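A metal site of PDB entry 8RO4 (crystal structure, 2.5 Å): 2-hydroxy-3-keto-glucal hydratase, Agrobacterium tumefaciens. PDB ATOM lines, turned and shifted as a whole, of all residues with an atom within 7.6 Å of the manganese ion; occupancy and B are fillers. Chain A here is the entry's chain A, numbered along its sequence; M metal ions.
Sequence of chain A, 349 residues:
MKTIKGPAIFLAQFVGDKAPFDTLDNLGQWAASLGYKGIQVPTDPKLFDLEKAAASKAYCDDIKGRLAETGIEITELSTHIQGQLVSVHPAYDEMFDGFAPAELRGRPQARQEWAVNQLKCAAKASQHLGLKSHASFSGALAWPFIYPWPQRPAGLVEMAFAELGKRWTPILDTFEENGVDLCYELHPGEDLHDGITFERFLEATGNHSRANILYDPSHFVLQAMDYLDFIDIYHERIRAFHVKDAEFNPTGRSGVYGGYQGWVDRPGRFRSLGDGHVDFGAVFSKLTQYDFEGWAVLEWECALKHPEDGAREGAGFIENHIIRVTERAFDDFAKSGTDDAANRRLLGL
The manganese ion is bound by OE2 of Glu 185, at 2.0 Å. The manganese ion is bound by the side-chain carboxylate (OD2) of Asp 216. The side-chain carboxylate (OE1) of Glu 299 binds the manganese ion, at 2.1 Å. ND1 of His 242 binds the manganese ion (2.1 Å).
Merely in contact with the manganese ion: His 219 (3.9 Å). Five residues have an atom within 4 Å of the manganese ion: Glu 185, Asp 216, His 219, His 242 and Glu 299. Along chain A the residues within 4 Å of the manganese ion span positions 185 to 299.
OE1 of Glu 185 sits at hydrogen-bond distance from NE2 of His 80. OG of Ser 218 is in hydrogen-bond range of OD1 of Asp 216, 2.8 Å away. The side-chain carboxylate (OE1) of Glu 299 lies close to the side-chain amino group (NZ) of Lys 244 (3.6 Å). The backbone NH (N) of Glu 299 lies within hydrogen-bond range of the backbone carbonyl oxygen (O) of Val 243 (3.3 Å). A ring nitrogen (NE2) of His 242 sits at hydrogen-bond distance from the side-chain amide oxygen (OE1) of Gln 40, at 2.9 Å. The backbone carbonyl oxygen (O) of Tyr 215 is in hydrogen-bond range of the backbone NH (N) of His 242 (2.9 Å).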
ATOM      1  N   PHE A  10     -23.229 -17.983  27.336  1.00  0.00           N
ATOM      2  CA  PHE A  10     -21.920 -17.692  26.760  1.00  0.00           C
ATOM      3  C   PHE A  10     -21.247 -16.613  27.601  1.00  0.00           C
ATOM      4  O   PHE A  10     -21.779 -15.505  27.755  1.00  0.00           O
ATOM      5  CB  PHE A  10     -22.091 -17.244  25.307  1.00  0.00           C
ATOM      6  CG  PHE A  10     -20.806 -17.155  24.523  1.00  0.00           C
ATOM      7  CD1 PHE A  10     -19.638 -17.747  24.984  1.00  0.00           C
ATOM      8  CD2 PHE A  10     -20.779 -16.488  23.302  1.00  0.00           C
ATOM      9  CE1 PHE A  10     -18.462 -17.669  24.254  1.00  0.00           C
ATOM     10  CE2 PHE A  10     -19.610 -16.415  22.569  1.00  0.00           C
ATOM     11  CZ  PHE A  10     -18.451 -17.004  23.041  1.00  0.00           C
ATOM     12  N   GLN A  13     -19.287 -12.185  26.945  1.00  0.00           N
ATOM     13  CA  GLN A  13     -19.790 -10.841  27.190  1.00  0.00           C
ATOM     14  C   GLN A  13     -19.770 -10.453  28.664  1.00  0.00           C
ATOM     15  O   GLN A  13     -20.106  -9.312  28.997  1.00  0.00           O
ATOM     16  CB  GLN A  13     -21.218 -10.708  26.662  1.00  0.00           C
ATOM     17  CG  GLN A  13     -21.306 -10.640  25.154  1.00  0.00           C
ATOM     18  CD  GLN A  13     -21.129 -11.996  24.499  1.00  0.00           C
ATOM     19  OE1 GLN A  13     -21.227 -13.034  25.162  1.00  0.00           O
ATOM     20  NE2 GLN A  13     -20.834 -12.000  23.202  1.00  0.00           N
ATOM     21  N   GLN A  40     -20.674 -21.820  27.637  1.00  0.00           N
ATOM     22  CA  GLN A  40     -19.801 -21.810  26.478  1.00  0.00           C
ATOM     23  C   GLN A  40     -18.581 -20.990  26.858  1.00  0.00           C
ATOM     24  O   GLN A  40     -18.715 -19.837  27.273  1.00  0.00           O
ATOM     25  CB  GLN A  40     -20.514 -21.220  25.252  1.00  0.00           C
ATOM     26  CG  GLN A  40     -20.068 -21.792  23.924  1.00  0.00           C
ATOM     27  CD  GLN A  40     -20.744 -21.129  22.735  1.00  0.00           C
ATOM     28  OE1 GLN A  40     -21.190 -19.986  22.820  1.00  0.00           O
ATOM     29  NE2 GLN A  40     -20.826 -21.848  21.618  1.00  0.00           N
ATOM     30  N   HIS A  80     -13.923 -17.915  18.476  1.00  0.00           N
ATOM     31  CA  HIS A  80     -14.342 -16.853  17.570  1.00  0.00           C
ATOM     32  C   HIS A  80     -13.180 -15.926  17.228  1.00  0.00           C
ATOM     33  O   HIS A  80     -12.978 -15.566  16.064  1.00  0.00           O
ATOM     34  CB  HIS A  80     -15.497 -16.061  18.177  1.00  0.00           C
ATOM     35  CG  HIS A  80     -16.793 -16.816  18.205  1.00  0.00           C
ATOM     36  ND1 HIS A  80     -17.242 -17.496  19.316  1.00  0.00           N
ATOM     37  CD2 HIS A  80     -17.747 -16.974  17.256  1.00  0.00           C
ATOM     38  CE1 HIS A  80     -18.398 -18.056  19.054  1.00  0.00           C
ATOM     39  NE2 HIS A  80     -18.738 -17.765  17.813  1.00  0.00           N
ATOM     40  N   PHE A 137     -15.381 -18.538  14.177  1.00  0.00           N
ATOM     41  CA  PHE A 137     -15.560 -17.685  13.008  1.00  0.00           C
ATOM     42  C   PHE A 137     -14.673 -18.199  11.877  1.00  0.00           C
ATOM     43  O   PHE A 137     -13.749 -18.992  12.094  1.00  0.00           O
ATOM     44  CB  PHE A 137     -15.204 -16.232  13.313  1.00  0.00           C
ATOM     45  CG  PHE A 137     -16.302 -15.449  13.981  1.00  0.00           C
ATOM     46  CD1 PHE A 137     -17.641 -15.690  13.687  1.00  0.00           C
ATOM     47  CD2 PHE A 137     -15.995 -14.451  14.890  1.00  0.00           C
ATOM     48  CE1 PHE A 137     -18.640 -14.956  14.297  1.00  0.00           C
ATOM     49  CE2 PHE A 137     -17.000 -13.709  15.502  1.00  0.00           C
ATOM     50  CZ  PHE A 137     -18.326 -13.965  15.204  1.00  0.00           C
ATOM     51  N   GLU A 185     -20.235 -19.562  12.798  1.00  0.00           N
ATOM     52  CA  GLU A 185     -21.329 -18.621  12.985  1.00  0.00           C
ATOM     53  C   GLU A 185     -21.367 -17.650  11.811  1.00  0.00           C
ATOM     54  O   GLU A 185     -20.425 -16.888  11.606  1.00  0.00           O
ATOM     55  CB  GLU A 185     -21.175 -17.859  14.307  1.00  0.00           C
ATOM     56  CG  GLU A 185     -22.357 -16.952  14.597  1.00  0.00           C
ATOM     57  CD  GLU A 185     -22.417 -16.503  16.039  1.00  0.00           C
ATOM     58  OE1 GLU A 185     -21.554 -16.932  16.831  1.00  0.00           O
ATOM     59  OE2 GLU A 185     -23.331 -15.730  16.373  1.00  0.00           O
ATOM     60  N   LEU A 186     -22.454 -17.702  11.047  1.00  0.00           N
ATOM     61  CA  LEU A 186     -22.615 -16.803   9.910  1.00  0.00           C
ATOM     62  C   LEU A 186     -22.861 -15.383  10.416  1.00  0.00           C
ATOM     63  O   LEU A 186     -23.867 -15.118  11.074  1.00  0.00           O
ATOM     64  CB  LEU A 186     -23.764 -17.284   9.025  1.00  0.00           C
ATOM     65  CG  LEU A 186     -23.651 -18.748   8.621  1.00  0.00           C
ATOM     66  CD1 LEU A 186     -24.754 -19.138   7.639  1.00  0.00           C
ATOM     67  CD2 LEU A 186     -22.279 -19.063   8.038  1.00  0.00           C
ATOM     68  N   HIS A 187     -21.947 -14.476  10.079  1.00  0.00           N
ATOM     69  CA  HIS A 187     -21.825 -13.202  10.773  1.00  0.00           C
ATOM     70  C   HIS A 187     -21.284 -12.176   9.787  1.00  0.00           C
ATOM     71  O   HIS A 187     -20.397 -12.516   8.990  1.00  0.00           O
ATOM     72  CB  HIS A 187     -20.875 -13.363  11.963  1.00  0.00           C
ATOM     73  CG  HIS A 187     -20.813 -12.182  12.873  1.00  0.00           C
ATOM     74  ND1 HIS A 187     -19.946 -11.124  12.665  1.00  0.00           N
ATOM     75  CD2 HIS A 187     -21.480 -11.902  14.021  1.00  0.00           C
ATOM     76  CE1 HIS A 187     -20.095 -10.239  13.636  1.00  0.00           C
ATOM     77  NE2 HIS A 187     -21.016 -10.677  14.470  1.00  0.00           N
ATOM     78  N   LEU A 214     -23.284 -22.803  13.283  1.00  0.00           N
ATOM     79  CA  LEU A 214     -23.856 -22.311  14.524  1.00  0.00           C
ATOM     80  C   LEU A 214     -24.973 -21.334  14.164  1.00  0.00           C
ATOM     81  O   LEU A 214     -24.720 -20.279  13.566  1.00  0.00           O
ATOM     82  CB  LEU A 214     -22.799 -21.640  15.405  1.00  0.00           C
ATOM     83  CG  LEU A 214     -23.116 -21.343  16.872  1.00  0.00           C
ATOM     84  CD1 LEU A 214     -21.834 -21.073  17.617  1.00  0.00           C
ATOM     85  CD2 LEU A 214     -24.073 -20.173  17.066  1.00  0.00           C
ATOM     86  N   TYR A 215     -26.212 -21.683  14.531  1.00  0.00           N
ATOM     87  CA  TYR A 215     -27.379 -20.900  14.149  1.00  0.00           C
ATOM     88  C   TYR A 215     -27.609 -19.775  15.160  1.00  0.00           C
ATOM     89  O   TYR A 215     -27.798 -20.027  16.359  1.00  0.00           O
ATOM     90  CB  TYR A 215     -28.607 -21.805  14.061  1.00  0.00           C
ATOM     91  CG  TYR A 215     -29.899 -21.088  13.740  1.00  0.00           C
ATOM     92  CD1 TYR A 215     -30.143 -20.576  12.464  1.00  0.00           C
ATOM     93  CD2 TYR A 215     -30.891 -20.933  14.706  1.00  0.00           C
ATOM     94  CE1 TYR A 215     -31.319 -19.929  12.167  1.00  0.00           C
ATOM     95  CE2 TYR A 215     -32.076 -20.295  14.414  1.00  0.00           C
ATOM     96  CZ  TYR A 215     -32.293 -19.787  13.141  1.00  0.00           C
ATOM     97  OH  TYR A 215     -33.470 -19.143  12.853  1.00  0.00           O
ATOM     98  N   ASP A 216     -27.599 -18.539  14.672  1.00  0.00           N
ATOM     99  CA  ASP A 216     -27.891 -17.353  15.467  1.00  0.00           C
ATOM    100  C   ASP A 216     -28.841 -16.478  14.667  1.00  0.00           C
ATOM    101  O   ASP A 216     -28.416 -15.795  13.718  1.00  0.00           O
ATOM    102  CB  ASP A 216     -26.613 -16.588  15.834  1.00  0.00           C
ATOM    103  CG  ASP A 216     -26.852 -15.469  16.841  1.00  0.00           C
ATOM    104  OD1 ASP A 216     -27.933 -14.848  16.834  1.00  0.00           O
ATOM    105  OD2 ASP A 216     -25.931 -15.209  17.652  1.00  0.00           O
ATOM    106  N   PRO A 217     -30.134 -16.447  15.028  1.00  0.00           N
ATOM    107  CA  PRO A 217     -31.113 -15.743  14.186  1.00  0.00           C
ATOM    108  C   PRO A 217     -30.965 -14.222  14.188  1.00  0.00           C
ATOM    109  O   PRO A 217     -31.502 -13.575  13.289  1.00  0.00           O
ATOM    110  CB  PRO A 217     -32.461 -16.175  14.775  1.00  0.00           C
ATOM    111  CG  PRO A 217     -32.147 -16.511  16.200  1.00  0.00           C
ATOM    112  CD  PRO A 217     -30.754 -17.084  16.193  1.00  0.00           C
ATOM    113  N   SER A 218     -30.265 -13.645  15.166  1.00  0.00           N
ATOM    114  CA  SER A 218     -30.188 -12.193  15.259  1.00  0.00           C
ATOM    115  C   SER A 218     -29.481 -11.580  14.055  1.00  0.00           C
ATOM    116  O   SER A 218     -29.886 -10.523  13.554  1.00  0.00           O
ATOM    117  CB  SER A 218     -29.474 -11.781  16.545  1.00  0.00           C
ATOM    118  OG  SER A 218     -28.088 -12.119  16.479  1.00  0.00           O
ATOM    119  N   HIS A 219     -28.424 -12.233  13.564  1.00  0.00           N
ATOM    120  CA  HIS A 219     -27.677 -11.675  12.443  1.00  0.00           C
ATOM    121  C   HIS A 219     -28.479 -11.736  11.155  1.00  0.00           C
ATOM    122  O   HIS A 219     -28.274 -10.905  10.261  1.00  0.00           O
ATOM    123  CB  HIS A 219     -26.360 -12.425  12.274  1.00  0.00           C
ATOM    124  CG  HIS A 219     -25.528 -12.433  13.518  1.00  0.00           C
ATOM    125  ND1 HIS A 219     -25.229 -13.587  14.202  1.00  0.00           N
ATOM    126  CD2 HIS A 219     -24.967 -11.422  14.223  1.00  0.00           C
ATOM    127  CE1 HIS A 219     -24.497 -13.298  15.265  1.00  0.00           C
ATOM    128  NE2 HIS A 219     -24.328 -11.982  15.307  1.00  0.00           N
ATOM    129  N   PHE A 241     -26.505 -23.609  18.692  1.00  0.00           N
ATOM    130  CA  PHE A 241     -27.635 -22.683  18.725  1.00  0.00           C
ATOM    131  C   PHE A 241     -27.340 -21.537  19.692  1.00  0.00           C
ATOM    132  O   PHE A 241     -27.136 -21.771  20.889  1.00  0.00           O
ATOM    133  CB  PHE A 241     -28.908 -23.442  19.138  1.00  0.00           C
ATOM    134  CG  PHE A 241     -30.142 -22.587  19.221  1.00  0.00           C
ATOM    135  CD1 PHE A 241     -30.295 -21.445  18.437  1.00  0.00           C
ATOM    136  CD2 PHE A 241     -31.174 -22.939  20.082  1.00  0.00           C
ATOM    137  CE1 PHE A 241     -31.434 -20.673  18.525  1.00  0.00           C
ATOM    138  CE2 PHE A 241     -32.321 -22.173  20.167  1.00  0.00           C
ATOM    139  CZ  PHE A 241     -32.448 -21.039  19.395  1.00  0.00           C
ATOM    140  N   HIS A 242     -27.335 -20.311  19.176  1.00  0.00           N
ATOM    141  CA  HIS A 242     -27.231 -19.110  19.991  1.00  0.00           C
ATOM    142  C   HIS A 242     -28.609 -18.462  20.108  1.00  0.00           C
ATOM    143  O   HIS A 242     -29.245 -18.158  19.096  1.00  0.00           O
ATOM    144  CB  HIS A 242     -26.245 -18.112  19.386  1.00  0.00           C
ATOM    145  CG  HIS A 242     -24.831 -18.280  19.855  1.00  0.00           C
ATOM    146  ND1 HIS A 242     -23.815 -17.436  19.476  1.00  0.00           N
ATOM    147  CD2 HIS A 242     -24.279 -19.189  20.693  1.00  0.00           C
ATOM    148  CE1 HIS A 242     -22.690 -17.817  20.048  1.00  0.00           C
ATOM    149  NE2 HIS A 242     -22.945 -18.874  20.798  1.00  0.00           N
ATOM    150  N   VAL A 243     -29.063 -18.240  21.335  1.00  0.00           N
ATOM    151  CA  VAL A 243     -30.326 -17.548  21.589  1.00  0.00           C
ATOM    152  C   VAL A 243     -30.025 -16.069  21.775  1.00  0.00           C
ATOM    153  O   VAL A 243     -29.493 -15.659  22.809  1.00  0.00           O
ATOM    154  CB  VAL A 243     -31.057 -18.118  22.806  1.00  0.00           C
ATOM    155  CG1 VAL A 243     -32.453 -17.525  22.875  1.00  0.00           C
ATOM    156  CG2 VAL A 243     -31.090 -19.636  22.748  1.00  0.00           C
ATOM    157  N   LYS A 244     -30.359 -15.266  20.766  1.00  0.00           N
ATOM    158  CA  LYS A 244     -30.026 -13.844  20.770  1.00  0.00           C
ATOM    159  C   LYS A 244     -31.092 -13.098  19.996  1.00  0.00           C
ATOM    160  O   LYS A 244     -31.492 -13.530  18.908  1.00  0.00           O
ATOM    161  CB  LYS A 244     -28.639 -13.636  20.151  1.00  0.00           C
ATOM    162  CG  LYS A 244     -28.074 -12.226  20.266  1.00  0.00           C
ATOM    163  CD  LYS A 244     -26.700 -12.166  19.617  1.00  0.00           C
ATOM    164  CE  LYS A 244     -25.948 -10.905  19.977  1.00  0.00           C
ATOM    165  NZ  LYS A 244     -24.660 -10.813  19.239  1.00  0.00           N
ATOM    166  N   PHE A 270     -29.316  -5.095  18.353  1.00  0.00           N
ATOM    167  CA  PHE A 270     -29.568  -6.216  19.251  1.00  0.00           C
ATOM    168  C   PHE A 270     -30.395  -5.777  20.449  1.00  0.00           C
ATOM    169  O   PHE A 270     -30.287  -4.642  20.931  1.00  0.00           O
ATOM    170  CB  PHE A 270     -28.248  -6.833  19.728  1.00  0.00           C
ATOM    171  CG  PHE A 270     -27.393  -7.354  18.622  1.00  0.00           C
ATOM    172  CD1 PHE A 270     -27.759  -8.496  17.918  1.00  0.00           C
ATOM    173  CD2 PHE A 270     -26.212  -6.717  18.285  1.00  0.00           C
ATOM    174  CE1 PHE A 270     -26.956  -8.977  16.896  1.00  0.00           C
ATOM    175  CE2 PHE A 270     -25.416  -7.191  17.265  1.00  0.00           C
ATOM    176  CZ  PHE A 270     -25.788  -8.325  16.563  1.00  0.00           C
ATOM    177  N   VAL A 297     -27.857 -21.883  23.924  1.00  0.00           N
ATOM    178  CA  VAL A 297     -26.858 -21.053  24.576  1.00  0.00           C
ATOM    179  C   VAL A 297     -27.259 -19.597  24.425  1.00  0.00           C
ATOM    180  O   VAL A 297     -27.390 -19.085  23.299  1.00  0.00           O
ATOM    181  CB  VAL A 297     -25.459 -21.292  23.985  1.00  0.00           C
ATOM    182  CG1 VAL A 297     -24.436 -20.415  24.682  1.00  0.00           C
ATOM    183  CG2 VAL A 297     -25.078 -22.756  24.108  1.00  0.00           C
ATOM    184  N   LEU A 298     -27.434 -18.908  25.552  1.00  0.00           N
ATOM    185  CA  LEU A 298     -27.747 -17.484  25.544  1.00  0.00           C
ATOM    186  C   LEU A 298     -26.486 -16.683  25.234  1.00  0.00           C
ATOM    187  O   LEU A 298     -25.465 -16.822  25.920  1.00  0.00           O
ATOM    188  CB  LEU A 298     -28.325 -17.052  26.891  1.00  0.00           C
ATOM    189  CG  LEU A 298     -28.309 -15.538  27.108  1.00  0.00           C
ATOM    190  CD1 LEU A 298     -29.296 -14.854  26.169  1.00  0.00           C
ATOM    191  CD2 LEU A 298     -28.623 -15.192  28.551  1.00  0.00           C
ATOM    192  N   GLU A 299     -26.547 -15.850  24.208  1.00  0.00           N
ATOM    193  CA  GLU A 299     -25.531 -14.847  23.927  1.00  0.00           C
ATOM    194  C   GLU A 299     -26.188 -13.478  24.101  1.00  0.00           C
ATOM    195  O   GLU A 299     -26.998 -13.070  23.254  1.00  0.00           O
ATOM    196  CB  GLU A 299     -24.940 -15.005  22.531  1.00  0.00           C
ATOM    197  CG  GLU A 299     -23.799 -14.045  22.243  1.00  0.00           C
ATOM    198  CD  GLU A 299     -23.241 -14.186  20.837  1.00  0.00           C
ATOM    199  OE1 GLU A 299     -24.026 -14.282  19.876  1.00  0.00           O
ATOM    200  OE2 GLU A 299     -22.000 -14.214  20.698  1.00  0.00           O
HETATM  201 MN    MN M   1     -24.012 -15.667  18.284  1.00  0.00          MN
